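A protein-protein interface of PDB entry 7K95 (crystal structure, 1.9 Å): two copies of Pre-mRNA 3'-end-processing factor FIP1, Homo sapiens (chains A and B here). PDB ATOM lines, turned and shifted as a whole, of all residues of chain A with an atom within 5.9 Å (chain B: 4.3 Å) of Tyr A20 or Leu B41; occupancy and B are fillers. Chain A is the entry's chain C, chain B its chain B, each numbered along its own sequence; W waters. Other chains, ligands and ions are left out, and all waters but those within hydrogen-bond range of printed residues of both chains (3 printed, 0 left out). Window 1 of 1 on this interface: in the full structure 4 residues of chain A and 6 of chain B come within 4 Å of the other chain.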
ATOM      1  N   PHE A  18      29.404 -12.810  19.628  1.00  0.00           N
ATOM      2  CA  PHE A  18      28.835 -13.321  20.896  1.00  0.00           C
ATOM      3  C   PHE A  18      29.437 -14.678  21.245  1.00  0.00           C
ATOM      4  O   PHE A  18      29.390 -15.579  20.402  1.00  0.00           O
ATOM      5  CB  PHE A  18      27.321 -13.487  20.824  1.00  0.00           C
ATOM      6  CG  PHE A  18      26.601 -12.188  20.671  1.00  0.00           C
ATOM      7  CD1 PHE A  18      26.374 -11.374  21.775  1.00  0.00           C
ATOM      8  CD2 PHE A  18      26.263 -11.713  19.418  1.00  0.00           C
ATOM      9  CE1 PHE A  18      25.684 -10.183  21.642  1.00  0.00           C
ATOM     10  CE2 PHE A  18      25.609 -10.497  19.285  1.00  0.00           C
ATOM     11  CZ  PHE A  18      25.354  -9.716  20.395  1.00  0.00           C
ATOM     12  N   ASN A  19      29.931 -14.802  22.482  1.00  0.00           N
ATOM     13  CA  ASN A  19      30.501 -16.076  22.960  1.00  0.00           C
ATOM     14  C   ASN A  19      29.351 -16.871  23.593  1.00  0.00           C
ATOM     15  O   ASN A  19      28.252 -16.289  23.854  1.00  0.00           O
ATOM     16  CB  ASN A  19      31.675 -15.847  23.907  1.00  0.00           C
ATOM     17  CG  ASN A  19      32.625 -17.033  24.053  1.00  0.00           C
ATOM     18  OD1 ASN A  19      32.325 -18.121  23.531  1.00  0.00           O
ATOM     19  ND2 ASN A  19      33.692 -16.830  24.841  1.00  0.00           N
ATOM     20  N   TYR A  20      29.581 -18.146  23.905  1.00  0.00           N
ATOM     21  CA  TYR A  20      28.695 -18.961  24.797  1.00  0.00           C
ATOM     22  C   TYR A  20      27.287 -19.219  24.220  1.00  0.00           C
ATOM     23  O   TYR A  20      26.438 -19.691  24.967  1.00  0.00           O
ATOM     24  CB  TYR A  20      28.629 -18.332  26.219  1.00  0.00           C
ATOM     25  CG  TYR A  20      29.948 -18.028  26.881  1.00  0.00           C
ATOM     26  CD1 TYR A  20      30.844 -19.041  27.225  1.00  0.00           C
ATOM     27  CD2 TYR A  20      30.388 -16.719  27.063  1.00  0.00           C
ATOM     28  CE1 TYR A  20      32.105 -18.768  27.717  1.00  0.00           C
ATOM     29  CE2 TYR A  20      31.636 -16.444  27.609  1.00  0.00           C
ATOM     30  CZ  TYR A  20      32.511 -17.472  27.965  1.00  0.00           C
ATOM     31  OH  TYR A  20      33.746 -17.168  28.467  1.00  0.00           O
ATOM     32  N   GLY A  21      27.053 -18.960  22.941  1.00  0.00           N
ATOM     33  CA  GLY A  21      25.752 -18.970  22.284  1.00  0.00           C
ATOM     34  C   GLY A  21      24.888 -17.802  22.704  1.00  0.00           C
ATOM     35  O   GLY A  21      23.644 -18.000  22.622  1.00  0.00           O
ATOM     36  N   PHE A  22      25.445 -16.687  23.198  1.00  0.00           N
ATOM     37  CA  PHE A  22      24.636 -15.458  23.442  1.00  0.00           C
ATOM     38  C   PHE A  22      24.109 -14.934  22.106  1.00  0.00           C
ATOM     39  O   PHE A  22      24.762 -15.194  21.033  1.00  0.00           O
ATOM     40  CB  PHE A  22      25.436 -14.336  24.119  1.00  0.00           C
ATOM     41  CG  PHE A  22      25.537 -14.443  25.621  1.00  0.00           C
ATOM     42  CD1 PHE A  22      24.430 -14.237  26.423  1.00  0.00           C
ATOM     43  CD2 PHE A  22      26.752 -14.658  26.241  1.00  0.00           C
ATOM     44  CE1 PHE A  22      24.535 -14.312  27.800  1.00  0.00           C
ATOM     45  CE2 PHE A  22      26.872 -14.686  27.617  1.00  0.00           C
ATOM     46  CZ  PHE A  22      25.753 -14.547  28.402  1.00  0.00           C
ATOM     47  N   THR A  26      19.683 -12.161  24.586  1.00  0.00           N
ATOM     48  CA  THR A  26      20.074 -12.841  25.844  1.00  0.00           C
ATOM     49  C   THR A  26      21.306 -12.144  26.470  1.00  0.00           C
ATOM     50  O   THR A  26      21.487 -12.217  27.699  1.00  0.00           O
ATOM     51  CB  THR A  26      20.347 -14.330  25.628  1.00  0.00           C
ATOM     52  OG1 THR A  26      21.276 -14.510  24.548  1.00  0.00           O
ATOM     53  CG2 THR A  26      19.051 -15.065  25.383  1.00  0.00           C
ATOM     54  N   TRP A  27      22.145 -11.508  25.657  1.00  0.00           N
ATOM     55  CA  TRP A  27      23.296 -10.729  26.190  1.00  0.00           C
ATOM     56  C   TRP A  27      22.737  -9.548  27.001  1.00  0.00           C
ATOM     57  O   TRP A  27      23.203  -9.307  28.139  1.00  0.00           O
ATOM     58  CB  TRP A  27      24.220 -10.276  25.061  1.00  0.00           C
ATOM     59  CG  TRP A  27      25.394  -9.492  25.558  1.00  0.00           C
ATOM     60  CD1 TRP A  27      25.691  -8.206  25.283  1.00  0.00           C
ATOM     61  CD2 TRP A  27      26.449  -9.984  26.411  1.00  0.00           C
ATOM     62  NE1 TRP A  27      26.829  -7.835  25.936  1.00  0.00           N
ATOM     63  CE2 TRP A  27      27.353  -8.923  26.581  1.00  0.00           C
ATOM     64  CE3 TRP A  27      26.746 -11.218  26.994  1.00  0.00           C
ATOM     65  CZ2 TRP A  27      28.511  -9.033  27.341  1.00  0.00           C
ATOM     66  CZ3 TRP A  27      27.901 -11.321  27.751  1.00  0.00           C
ATOM     67  CH2 TRP A  27      28.756 -10.240  27.924  1.00  0.00           C
ATOM     68  N   LYS B  33      33.050 -22.626  33.440  1.00  0.00           N
ATOM     69  CA  LYS B  33      32.413 -21.336  33.018  1.00  0.00           C
ATOM     70  C   LYS B  33      31.590 -21.548  31.755  1.00  0.00           C
ATOM     71  O   LYS B  33      30.437 -21.078  31.726  1.00  0.00           O
ATOM     72  CB  LYS B  33      33.454 -20.231  32.888  1.00  0.00           C
ATOM     73  CG  LYS B  33      32.937 -19.005  32.146  1.00  0.00           C
ATOM     74  CD  LYS B  33      33.989 -17.948  31.879  1.00  0.00           C
ATOM     75  CE  LYS B  33      34.469 -17.314  33.175  1.00  0.00           C
ATOM     76  NZ  LYS B  33      35.738 -16.571  32.938  1.00  0.00           N
ATOM     77  N   GLN B  34      32.161 -22.215  30.724  1.00  0.00           N
ATOM     78  CA  GLN B  34      31.385 -22.558  29.510  1.00  0.00           C
ATOM     79  C   GLN B  34      30.080 -23.189  29.931  1.00  0.00           C
ATOM     80  O   GLN B  34      29.038 -22.869  29.327  1.00  0.00           O
ATOM     81  CB  GLN B  34      32.207 -23.519  28.668  1.00  0.00           C
ATOM     82  CG  GLN B  34      33.405 -22.858  28.041  1.00  0.00           C
ATOM     83  CD  GLN B  34      33.124 -22.121  26.760  1.00  0.00           C
ATOM     84  OE1 GLN B  34      32.006 -22.129  26.227  1.00  0.00           O
ATOM     85  NE2 GLN B  34      34.144 -21.398  26.257  1.00  0.00           N
ATOM     86  N   ILE B  37      27.484 -20.737  31.917  1.00  0.00           N
ATOM     87  CA  ILE B  37      26.863 -19.649  31.113  1.00  0.00           C
ATOM     88  C   ILE B  37      25.944 -20.319  30.090  1.00  0.00           C
ATOM     89  O   ILE B  37      24.802 -19.884  29.937  1.00  0.00           O
ATOM     90  CB  ILE B  37      27.981 -18.799  30.465  1.00  0.00           C
ATOM     91  CG1 ILE B  37      28.835 -18.141  31.552  1.00  0.00           C
ATOM     92  CG2 ILE B  37      27.379 -17.803  29.478  1.00  0.00           C
ATOM     93  CD1 ILE B  37      29.968 -17.282  31.059  1.00  0.00           C
ATOM     94  N   ARG B  38      26.395 -21.390  29.421  1.00  0.00           N
ATOM     95  CA  ARG B  38      25.610 -21.947  28.260  1.00  0.00           C
ATOM     96  C   ARG B  38      24.258 -22.527  28.678  1.00  0.00           C
ATOM     97  O   ARG B  38      23.288 -22.492  27.823  1.00  0.00           O
ATOM     98  CB  ARG B  38      26.399 -22.986  27.480  1.00  0.00           C
ATOM     99  CG  ARG B  38      27.491 -22.351  26.635  1.00  0.00           C
ATOM    100  CD  ARG B  38      28.314 -23.517  26.072  1.00  0.00           C
ATOM    101  NE  ARG B  38      29.468 -23.005  25.415  1.00  0.00           N
ATOM    102  CZ  ARG B  38      29.518 -22.558  24.201  1.00  0.00           C
ATOM    103  NH1 ARG B  38      28.443 -22.600  23.440  1.00  0.00           N
ATOM    104  NH2 ARG B  38      30.639 -21.959  23.767  1.00  0.00           N
ATOM    105  N   MET B  39      24.164 -23.055  29.893  1.00  0.00           N
ATOM    106  CA  MET B  39      22.956 -23.804  30.277  1.00  0.00           C
ATOM    107  C   MET B  39      21.707 -22.885  30.215  1.00  0.00           C
ATOM    108  O   MET B  39      20.545 -23.369  29.958  1.00  0.00           O
ATOM    109  CB  MET B  39      23.181 -24.348  31.680  1.00  0.00           C
ATOM    110  CG  MET B  39      23.503 -25.843  31.574  1.00  0.00           C
ATOM    111  SD  MET B  39      24.164 -26.261  33.093  1.00  0.00           S
ATOM    112  CE  MET B  39      22.635 -26.834  33.842  1.00  0.00           C
ATOM    113  N   GLY B  40      21.902 -21.583  30.458  1.00  0.00           N
ATOM    114  CA  GLY B  40      20.779 -20.636  30.589  1.00  0.00           C
ATOM    115  C   GLY B  40      20.417 -19.925  29.286  1.00  0.00           C
ATOM    116  O   GLY B  40      19.639 -18.933  29.385  1.00  0.00           O
ATOM    117  N   LEU B  41      20.959 -20.352  28.133  1.00  0.00           N
ATOM    118  CA  LEU B  41      20.810 -19.642  26.819  1.00  0.00           C
ATOM    119  C   LEU B  41      20.105 -20.502  25.741  1.00  0.00           C
ATOM    120  O   LEU B  41      20.061 -21.733  25.911  1.00  0.00           O
ATOM    121  CB  LEU B  41      22.193 -19.210  26.347  1.00  0.00           C
ATOM    122  CG  LEU B  41      22.916 -18.271  27.308  1.00  0.00           C
ATOM    123  CD1 LEU B  41      24.275 -17.953  26.729  1.00  0.00           C
ATOM    124  CD2 LEU B  41      22.103 -17.011  27.494  1.00  0.00           C
ATOM    125  N   GLU B  42      19.557 -19.836  24.698  1.00  0.00           N
ATOM    126  CA  GLU B  42      18.547 -20.369  23.740  1.00  0.00           C
ATOM    127  C   GLU B  42      19.183 -20.658  22.375  1.00  0.00           C
ATOM    128  O   GLU B  42      18.270 -20.904  21.511  1.00  0.00           O
ATOM    129  CB  GLU B  42      17.394 -19.368  23.595  1.00  0.00           C
ATOM    130  CG  GLU B  42      16.900 -18.809  24.919  1.00  0.00           C
ATOM    131  CD  GLU B  42      15.791 -17.793  24.763  1.00  0.00           C
ATOM    132  OE1 GLU B  42      15.950 -16.870  23.933  1.00  0.00           O
ATOM    133  OE2 GLU B  42      14.759 -17.965  25.433  1.00  0.00           O
HETATM  134  O   HOH W   1      21.245 -17.007  23.540  1.00  0.00           O
HETATM  135  O   HOH W   2      33.798 -20.453  23.474  1.00  0.00           O
HETATM  136  O   HOH W   3      24.388 -21.559  24.653  1.00  0.00           O
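The side-chain amide oxygen of Gln B34 lies within hydrogen-bond range of the guanidinium group of Arg B38, at 2.8 Å.
OH of Tyr A20 touches CD of Lys B33, at 3.5 Å.
CD1 of Tyr A20 touches OE1 of Gln B34, 3.4 Å away.
Ile B37 touches Tyr A20.
Arg B38 touches Tyr A20.
Tyr A20 touches Leu B41.
Arg B38 touches Gly A21 (NH1 to N, 3.9 Å).
Phe A22 touches Ile B37 (CE2 to CG2, 3.7 Å).
CE1 of Phe A22 touches CD2 of Leu B41 (3.6 Å).
Thr A26 touches Leu B41.
CG2 of Thr A26 touches OE1 of Glu B42, 3.9 Å away.
Of the printed residues of chain B, Phe A22 touches Ile B37 (3.7 Å) and Leu B41 (3.6 Å).
Printed residues of chain B within 4 Å of Thr A26: Leu B41 and Glu B42.
Printed residues of chain A within 4 Å of Lys B33: Tyr A20 (3.5 Å).
Of the printed residues of chain A, Gln B34 touches Tyr A20 (3.4 Å).
Gly B40 touches none of the printed residues of chain A.
Leu B41 touches just these residues of chain A: Tyr A20, Phe A22 and Thr A26.
Printed residues of chain A within 4 Å of Glu B42: Thr A26 (3.9 Å).
The nearest printed residue of chain B that does not touch Tyr A20 is Met B39 (6.4 Å).
Of the 7 printed residues of chain A, 4 touch a printed residue of chain B.
Of the 8 printed residues of chain B, 6 touch a printed residue of chain A.
Hydrophobic or aromatic side chains of chain B that line the printed part of chain A: Ile B37 and Leu B41.
Among the printed residues, no Asp or Glu carboxylate lies within 4 Å of a Lys or Arg side-chain nitrogen of the other chain.
No position is printed for both chains.
Of the 10 pairs that touch across the chains among the printed residues, none has its exchanged pair printed and touching as well.
Water W1 lies within hydrogen-bond range of OG1 of Thr A26 (2.7 Å), O of Gly A21 (2.8 Å) and N of Glu B42 (3.5 Å).
Water W2 lies within hydrogen-bond range of the side-chain amide oxygen of Asn A19 and the side-chain amide nitrogen of Gln B34.
Water W3 lies within hydrogen-bond range of O of Tyr A20 (2.8 Å) and O of Arg B38 (3.5 Å).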
